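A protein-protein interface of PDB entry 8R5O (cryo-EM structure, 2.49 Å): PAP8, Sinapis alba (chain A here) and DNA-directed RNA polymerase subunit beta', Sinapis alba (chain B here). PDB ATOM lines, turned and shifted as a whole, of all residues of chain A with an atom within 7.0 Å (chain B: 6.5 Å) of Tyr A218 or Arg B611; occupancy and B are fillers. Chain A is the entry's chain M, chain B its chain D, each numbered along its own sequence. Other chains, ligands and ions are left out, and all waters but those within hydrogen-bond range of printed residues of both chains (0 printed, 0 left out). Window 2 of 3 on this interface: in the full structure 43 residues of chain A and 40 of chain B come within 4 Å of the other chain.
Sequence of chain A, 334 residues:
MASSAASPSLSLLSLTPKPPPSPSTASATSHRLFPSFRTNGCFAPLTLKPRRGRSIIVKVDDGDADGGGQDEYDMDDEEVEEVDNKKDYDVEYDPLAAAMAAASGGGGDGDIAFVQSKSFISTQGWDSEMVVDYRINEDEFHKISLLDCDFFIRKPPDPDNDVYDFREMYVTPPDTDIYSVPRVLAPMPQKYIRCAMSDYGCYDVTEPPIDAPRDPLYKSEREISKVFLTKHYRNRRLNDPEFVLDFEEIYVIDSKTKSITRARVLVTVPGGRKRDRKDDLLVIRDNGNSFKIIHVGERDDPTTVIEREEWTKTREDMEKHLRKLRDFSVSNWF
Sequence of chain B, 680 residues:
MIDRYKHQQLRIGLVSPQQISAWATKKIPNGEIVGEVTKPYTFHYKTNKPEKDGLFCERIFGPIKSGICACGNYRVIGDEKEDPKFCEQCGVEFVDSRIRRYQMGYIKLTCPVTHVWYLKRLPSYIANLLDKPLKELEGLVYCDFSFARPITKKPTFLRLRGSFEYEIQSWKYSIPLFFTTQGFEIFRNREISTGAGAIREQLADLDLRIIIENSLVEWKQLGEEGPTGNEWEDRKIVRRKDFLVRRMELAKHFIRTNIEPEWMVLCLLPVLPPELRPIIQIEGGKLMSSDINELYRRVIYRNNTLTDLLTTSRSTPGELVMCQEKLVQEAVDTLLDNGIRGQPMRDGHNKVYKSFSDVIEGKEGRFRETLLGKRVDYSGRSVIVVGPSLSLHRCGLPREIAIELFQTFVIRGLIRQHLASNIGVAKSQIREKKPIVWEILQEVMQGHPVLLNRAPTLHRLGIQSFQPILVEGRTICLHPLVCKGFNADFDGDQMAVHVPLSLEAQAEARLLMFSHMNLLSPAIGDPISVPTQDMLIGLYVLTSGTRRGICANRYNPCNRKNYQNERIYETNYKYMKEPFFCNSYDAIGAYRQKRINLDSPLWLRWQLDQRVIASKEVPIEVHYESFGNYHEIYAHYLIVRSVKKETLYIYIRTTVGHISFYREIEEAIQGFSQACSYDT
OH of Tyr A218 sits at hydrogen-bond distance from OD2 of Asp B609 (2.6 Å).
The side-chain hydroxyl (OH) of Tyr A218 is in hydrogen-bond range of the guanidinium group (NH2) of Arg B611 (2.9 Å).
The side-chain hydroxyl of Ser A220 is in hydrogen-bond range of the backbone carbonyl oxygen of Gln B610.
The indole nitrogen (NE1) of Trp B606 sits at hydrogen-bond distance from the backbone carbonyl oxygen (O) of Asp B609, at 2.6 Å.
The side-chain carboxylate (OD1) of Asp B609 lies within salt-bridge range of the guanidinium group (NE) of Arg B611.
The side-chain amide oxygen (OE1) of Gln B610 sits at hydrogen-bond distance from the backbone NH (N) of Val B612 (3.1 Å).
NH1 of Arg B611 is in hydrogen-bond range of OH of Tyr B662, 3.1 Å away.
Tyr A203 touches Gln B610.
Val A205 touches Gln B610.
Val A205 touches Val B612 (CG2 to O, 3.7 Å).
Val A205 touches Ile B613.
Tyr A218 touches just these residues of chain B: Asp B609 and Arg B611.
Of chain A, only Tyr A218 (2.9 Å) comes within 4 Å of Arg B611.
Of the printed residues of chain B, Val A205 touches Gln B610 (3.6 Å), Val B612 (3.7 Å) and Ile B613 (3.3 Å).
Printed residues of chain A within 4 Å of Val B612: Val A205 (3.7 Å).
Printed residues of chain A within 4 Å of Gln B610: Tyr A203 (3.4 Å), Val A205 (3.6 Å) and Ser A220 (2.5 Å).
Of the printed residues of chain B, Ser A220 touches Gln B610 (2.5 Å).
The nearest residue of chain B that does not touch Tyr A218 is Gln B610 (5.0 Å).
The nearest residue of chain A that does not touch Arg B611 is Val A205 (4.1 Å).
The nearest printed residue of chain A that does not touch Gln B610 is Tyr A218 (5.0 Å).
Hydrophobic or aromatic side chains of chain B that line the printed part of chain A: Ile B613.
Along chain B the printed residues that touch a printed residue of chain A span positions 609 to 613.
Of the 11 printed residues of chain A, 4 touch a printed residue of chain B.
Hydrophobic or aromatic side chains of chain A that line the printed part of chain B: Tyr A203, Val A205 and Tyr A218.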
ATOM      1  N   TYR A 203      28.839 -24.043  -1.560  1.00  0.00           N
ATOM      2  CA  TYR A 203      29.524 -23.062  -0.731  1.00  0.00           C
ATOM      3  C   TYR A 203      29.861 -23.683   0.615  1.00  0.00           C
ATOM      4  O   TYR A 203      28.998 -24.291   1.257  1.00  0.00           O
ATOM      5  CB  TYR A 203      28.668 -21.815  -0.523  1.00  0.00           C
ATOM      6  CG  TYR A 203      28.547 -20.941  -1.741  1.00  0.00           C
ATOM      7  CD1 TYR A 203      27.589 -21.198  -2.706  1.00  0.00           C
ATOM      8  CD2 TYR A 203      29.389 -19.853  -1.925  1.00  0.00           C
ATOM      9  CE1 TYR A 203      27.472 -20.403  -3.816  1.00  0.00           C
ATOM     10  CE2 TYR A 203      29.275 -19.048  -3.035  1.00  0.00           C
ATOM     11  CZ  TYR A 203      28.312 -19.328  -3.980  1.00  0.00           C
ATOM     12  OH  TYR A 203      28.189 -18.534  -5.094  1.00  0.00           O
ATOM     13  N   VAL A 205      30.506 -22.370   3.862  1.00  0.00           N
ATOM     14  CA  VAL A 205      30.422 -21.224   4.759  1.00  0.00           C
ATOM     15  C   VAL A 205      30.656 -21.739   6.172  1.00  0.00           C
ATOM     16  O   VAL A 205      29.822 -22.457   6.729  1.00  0.00           O
ATOM     17  CB  VAL A 205      29.074 -20.503   4.642  1.00  0.00           C
ATOM     18  CG1 VAL A 205      28.987 -19.376   5.659  1.00  0.00           C
ATOM     19  CG2 VAL A 205      28.880 -19.968   3.236  1.00  0.00           C
ATOM     20  N   THR A 206      31.796 -21.380   6.749  1.00  0.00           N
ATOM     21  CA  THR A 206      32.189 -21.827   8.075  1.00  0.00           C
ATOM     22  C   THR A 206      32.318 -20.639   9.018  1.00  0.00           C
ATOM     23  O   THR A 206      32.245 -19.477   8.612  1.00  0.00           O
ATOM     24  CB  THR A 206      33.510 -22.603   8.016  1.00  0.00           C
ATOM     25  OG1 THR A 206      34.507 -21.802   7.370  1.00  0.00           O
ATOM     26  CG2 THR A 206      33.332 -23.899   7.244  1.00  0.00           C
ATOM     27  N   GLU A 207      32.501 -20.950  10.302  1.00  0.00           N
ATOM     28  CA  GLU A 207      32.825 -19.964  11.333  1.00  0.00           C
ATOM     29  C   GLU A 207      34.142 -20.395  11.961  1.00  0.00           C
ATOM     30  O   GLU A 207      34.158 -21.189  12.916  1.00  0.00           O
ATOM     31  CB  GLU A 207      31.715 -19.849  12.377  1.00  0.00           C
ATOM     32  CG  GLU A 207      30.396 -19.316  11.837  1.00  0.00           C
ATOM     33  CD  GLU A 207      29.704 -18.368  12.804  1.00  0.00           C
ATOM     34  OE1 GLU A 207      30.275 -17.298  13.108  1.00  0.00           O
ATOM     35  OE2 GLU A 207      28.590 -18.695  13.265  1.00  0.00           O
ATOM     36  N   PRO A 208      35.270 -19.910  11.452  1.00  0.00           N
ATOM     37  CA  PRO A 208      36.572 -20.379  11.929  1.00  0.00           C
ATOM     38  C   PRO A 208      36.854 -19.872  13.331  1.00  0.00           C
ATOM     39  O   PRO A 208      36.284 -18.858  13.760  1.00  0.00           O
ATOM     40  CB  PRO A 208      37.561 -19.781  10.914  1.00  0.00           C
ATOM     41  CG  PRO A 208      36.716 -19.193   9.809  1.00  0.00           C
ATOM     42  CD  PRO A 208      35.403 -18.864  10.429  1.00  0.00           C
ATOM     43  N   ASP A 215      39.917 -11.341  13.823  1.00  0.00           N
ATOM     44  CA  ASP A 215      39.753 -12.511  12.974  1.00  0.00           C
ATOM     45  C   ASP A 215      38.312 -12.575  12.470  1.00  0.00           C
ATOM     46  O   ASP A 215      37.379 -12.276  13.224  1.00  0.00           O
ATOM     47  CB  ASP A 215      40.105 -13.789  13.734  1.00  0.00           C
ATOM     48  CG  ASP A 215      41.519 -14.259  13.463  1.00  0.00           C
ATOM     49  OD1 ASP A 215      42.219 -13.615  12.655  1.00  0.00           O
ATOM     50  OD2 ASP A 215      41.928 -15.278  14.054  1.00  0.00           O
ATOM     51  N   PRO A 216      38.096 -12.954  11.212  1.00  0.00           N
ATOM     52  CA  PRO A 216      36.745 -12.882  10.643  1.00  0.00           C
ATOM     53  C   PRO A 216      35.774 -13.812  11.355  1.00  0.00           C
ATOM     54  O   PRO A 216      36.141 -14.882  11.842  1.00  0.00           O
ATOM     55  CB  PRO A 216      36.953 -13.302   9.184  1.00  0.00           C
ATOM     56  CG  PRO A 216      38.187 -14.134   9.213  1.00  0.00           C
ATOM     57  CD  PRO A 216      39.065 -13.517  10.258  1.00  0.00           C
ATOM     58  N   LEU A 217      34.515 -13.382  11.412  1.00  0.00           N
ATOM     59  CA  LEU A 217      33.477 -14.188  12.044  1.00  0.00           C
ATOM     60  C   LEU A 217      33.063 -15.370  11.177  1.00  0.00           C
ATOM     61  O   LEU A 217      32.626 -16.395  11.708  1.00  0.00           O
ATOM     62  CB  LEU A 217      32.264 -13.317  12.371  1.00  0.00           C
ATOM     63  CG  LEU A 217      32.473 -12.329  13.519  1.00  0.00           C
ATOM     64  CD1 LEU A 217      31.299 -11.377  13.628  1.00  0.00           C
ATOM     65  CD2 LEU A 217      32.674 -13.077  14.824  1.00  0.00           C
ATOM     66  N   TYR A 218      33.193 -15.253   9.859  1.00  0.00           N
ATOM     67  CA  TYR A 218      32.854 -16.341   8.956  1.00  0.00           C
ATOM     68  C   TYR A 218      33.864 -16.393   7.822  1.00  0.00           C
ATOM     69  O   TYR A 218      34.607 -15.441   7.576  1.00  0.00           O
ATOM     70  CB  TYR A 218      31.438 -16.195   8.382  1.00  0.00           C
ATOM     71  CG  TYR A 218      31.277 -15.033   7.426  1.00  0.00           C
ATOM     72  CD1 TYR A 218      30.973 -13.763   7.894  1.00  0.00           C
ATOM     73  CD2 TYR A 218      31.422 -15.209   6.056  1.00  0.00           C
ATOM     74  CE1 TYR A 218      30.825 -12.701   7.026  1.00  0.00           C
ATOM     75  CE2 TYR A 218      31.279 -14.153   5.182  1.00  0.00           C
ATOM     76  CZ  TYR A 218      30.978 -12.901   5.672  1.00  0.00           C
ATOM     77  OH  TYR A 218      30.831 -11.845   4.805  1.00  0.00           O
ATOM     78  N   LYS A 219      33.877 -17.529   7.130  1.00  0.00           N
ATOM     79  CA  LYS A 219      34.664 -17.702   5.919  1.00  0.00           C
ATOM     80  C   LYS A 219      33.806 -18.419   4.891  1.00  0.00           C
ATOM     81  O   LYS A 219      33.269 -19.493   5.170  1.00  0.00           O
ATOM     82  CB  LYS A 219      35.949 -18.488   6.200  1.00  0.00           C
ATOM     83  CG  LYS A 219      36.747 -18.846   4.961  1.00  0.00           C
ATOM     84  CD  LYS A 219      38.166 -19.247   5.330  1.00  0.00           C
ATOM     85  CE  LYS A 219      38.857 -19.970   4.188  1.00  0.00           C
ATOM     86  NZ  LYS A 219      38.334 -21.354   4.020  1.00  0.00           N
ATOM     87  N   SER A 220      33.679 -17.825   3.708  1.00  0.00           N
ATOM     88  CA  SER A 220      32.800 -18.333   2.660  1.00  0.00           C
ATOM     89  C   SER A 220      33.636 -18.644   1.428  1.00  0.00           C
ATOM     90  O   SER A 220      34.166 -17.732   0.784  1.00  0.00           O
ATOM     91  CB  SER A 220      31.702 -17.322   2.337  1.00  0.00           C
ATOM     92  OG  SER A 220      30.829 -17.817   1.339  1.00  0.00           O
ATOM     93  N   TRP B 606      19.474 -10.659  -2.224  1.00  0.00           N
ATOM     94  CA  TRP B 606      20.695 -10.556  -1.437  1.00  0.00           C
ATOM     95  C   TRP B 606      21.754  -9.845  -2.264  1.00  0.00           C
ATOM     96  O   TRP B 606      22.093 -10.295  -3.362  1.00  0.00           O
ATOM     97  CB  TRP B 606      21.177 -11.941  -1.006  1.00  0.00           C
ATOM     98  CG  TRP B 606      22.272 -11.922   0.004  1.00  0.00           C
ATOM     99  CD1 TRP B 606      23.569 -12.292  -0.187  1.00  0.00           C
ATOM    100  CD2 TRP B 606      22.169 -11.512   1.371  1.00  0.00           C
ATOM    101  NE1 TRP B 606      24.280 -12.142   0.975  1.00  0.00           N
ATOM    102  CE2 TRP B 606      23.443 -11.664   1.948  1.00  0.00           C
ATOM    103  CE3 TRP B 606      21.122 -11.033   2.163  1.00  0.00           C
ATOM    104  CZ2 TRP B 606      23.700 -11.351   3.280  1.00  0.00           C
ATOM    105  CZ3 TRP B 606      21.378 -10.725   3.484  1.00  0.00           C
ATOM    106  CH2 TRP B 606      22.657 -10.886   4.030  1.00  0.00           C
ATOM    107  N   LEU B 608      24.869  -8.872  -0.889  1.00  0.00           N
ATOM    108  CA  LEU B 608      26.147  -9.040  -0.214  1.00  0.00           C
ATOM    109  C   LEU B 608      26.788 -10.337  -0.702  1.00  0.00           C
ATOM    110  O   LEU B 608      26.316 -10.967  -1.650  1.00  0.00           O
ATOM    111  CB  LEU B 608      25.966  -9.036   1.305  1.00  0.00           C
ATOM    112  CG  LEU B 608      25.450  -7.743   1.936  1.00  0.00           C
ATOM    113  CD1 LEU B 608      25.345  -7.893   3.444  1.00  0.00           C
ATOM    114  CD2 LEU B 608      26.356  -6.585   1.573  1.00  0.00           C
ATOM    115  N   ASP B 609      27.878 -10.731  -0.051  1.00  0.00           N
ATOM    116  CA  ASP B 609      28.490 -12.013  -0.354  1.00  0.00           C
ATOM    117  C   ASP B 609      27.646 -13.150   0.222  1.00  0.00           C
ATOM    118  O   ASP B 609      26.743 -12.946   1.036  1.00  0.00           O
ATOM    119  CB  ASP B 609      29.915 -12.072   0.192  1.00  0.00           C
ATOM    120  CG  ASP B 609      29.967 -11.914   1.697  1.00  0.00           C
ATOM    121  OD1 ASP B 609      29.187 -11.104   2.238  1.00  0.00           O
ATOM    122  OD2 ASP B 609      30.783 -12.602   2.341  1.00  0.00           O
ATOM    123  N   GLN B 610      27.954 -14.368  -0.218  1.00  0.00           N
ATOM    124  CA  GLN B 610      27.230 -15.564   0.210  1.00  0.00           C
ATOM    125  C   GLN B 610      27.714 -15.945   1.605  1.00  0.00           C
ATOM    126  O   GLN B 610      28.692 -16.672   1.777  1.00  0.00           O
ATOM    127  CB  GLN B 610      27.428 -16.692  -0.795  1.00  0.00           C
ATOM    128  CG  GLN B 610      26.966 -18.062  -0.325  1.00  0.00           C
ATOM    129  CD  GLN B 610      25.526 -18.083   0.114  1.00  0.00           C
ATOM    130  OE1 GLN B 610      25.226 -18.364   1.271  1.00  0.00           O
ATOM    131  NE2 GLN B 610      24.622 -17.795  -0.812  1.00  0.00           N
ATOM    132  N   ARG B 611      27.021 -15.437   2.620  1.00  0.00           N
ATOM    133  CA  ARG B 611      27.399 -15.637   4.013  1.00  0.00           C
ATOM    134  C   ARG B 611      26.310 -16.365   4.795  1.00  0.00           C
ATOM    135  O   ARG B 611      26.141 -16.139   5.993  1.00  0.00           O
ATOM    136  CB  ARG B 611      27.725 -14.300   4.677  1.00  0.00           C
ATOM    137  CG  ARG B 611      26.579 -13.309   4.638  1.00  0.00           C
ATOM    138  CD  ARG B 611      26.902 -12.043   5.403  1.00  0.00           C
ATOM    139  NE  ARG B 611      27.911 -11.234   4.732  1.00  0.00           N
ATOM    140  CZ  ARG B 611      28.315 -10.046   5.155  1.00  0.00           C
ATOM    141  NH1 ARG B 611      27.817  -9.497   6.250  1.00  0.00           N
ATOM    142  NH2 ARG B 611      29.243  -9.392   4.463  1.00  0.00           N
ATOM    143  N   VAL B 612      25.565 -17.240   4.133  1.00  0.00           N
ATOM    144  CA  VAL B 612      24.458 -17.947   4.766  1.00  0.00           C
ATOM    145  C   VAL B 612      24.951 -19.308   5.236  1.00  0.00           C
ATOM    146  O   VAL B 612      25.394 -20.130   4.428  1.00  0.00           O
ATOM    147  CB  VAL B 612      23.271 -18.094   3.804  1.00  0.00           C
ATOM    148  CG1 VAL B 612      22.083 -18.717   4.515  1.00  0.00           C
ATOM    149  CG2 VAL B 612      22.903 -16.748   3.221  1.00  0.00           C
ATOM    150  N   ILE B 613      24.879 -19.542   6.545  1.00  0.00           N
ATOM    151  CA  ILE B 613      25.213 -20.853   7.086  1.00  0.00           C
ATOM    152  C   ILE B 613      24.186 -21.860   6.590  1.00  0.00           C
ATOM    153  O   ILE B 613      22.983 -21.720   6.845  1.00  0.00           O
ATOM    154  CB  ILE B 613      25.264 -20.816   8.616  1.00  0.00           C
ATOM    155  CG1 ILE B 613      26.524 -20.097   9.094  1.00  0.00           C
ATOM    156  CG2 ILE B 613      25.218 -22.221   9.177  1.00  0.00           C
ATOM    157  CD1 ILE B 613      27.799 -20.843   8.795  1.00  0.00           C
ATOM    158  N   TYR B 662      19.013 -11.148  12.433  1.00  0.00           N
ATOM    159  CA  TYR B 662      20.213 -10.614  11.797  1.00  0.00           C
ATOM    160  C   TYR B 662      20.258  -9.095  11.890  1.00  0.00           C
ATOM    161  O   TYR B 662      21.317  -8.513  12.153  1.00  0.00           O
ATOM    162  CB  TYR B 662      20.270 -11.064  10.339  1.00  0.00           C
ATOM    163  CG  TYR B 662      21.557 -10.709   9.639  1.00  0.00           C
ATOM    164  CD1 TYR B 662      22.704 -11.461   9.838  1.00  0.00           C
ATOM    165  CD2 TYR B 662      21.625  -9.629   8.771  1.00  0.00           C
ATOM    166  CE1 TYR B 662      23.884 -11.146   9.201  1.00  0.00           C
ATOM    167  CE2 TYR B 662      22.804  -9.306   8.128  1.00  0.00           C
ATOM    168  CZ  TYR B 662      23.928 -10.070   8.347  1.00  0.00           C
ATOM    169  OH  TYR B 662      25.107  -9.759   7.709  1.00  0.00           O
ATOM    170  N   GLU B 666      23.093  -6.574  13.740  1.00  0.00           N
ATOM    171  CA  GLU B 666      23.787  -5.649  12.849  1.00  0.00           C
ATOM    172  C   GLU B 666      23.526  -4.200  13.240  1.00  0.00           C
ATOM    173  O   GLU B 666      24.455  -3.387  13.285  1.00  0.00           O
ATOM    174  CB  GLU B 666      23.369  -5.894  11.400  1.00  0.00           C
ATOM    175  CG  GLU B 666      24.123  -5.027  10.403  1.00  0.00           C
ATOM    176  CD  GLU B 666      23.751  -5.319   8.966  1.00  0.00           C
ATOM    177  OE1 GLU B 666      22.818  -6.118   8.739  1.00  0.00           O
ATOM    178  OE2 GLU B 666      24.392  -4.750   8.059  1.00  0.00           O
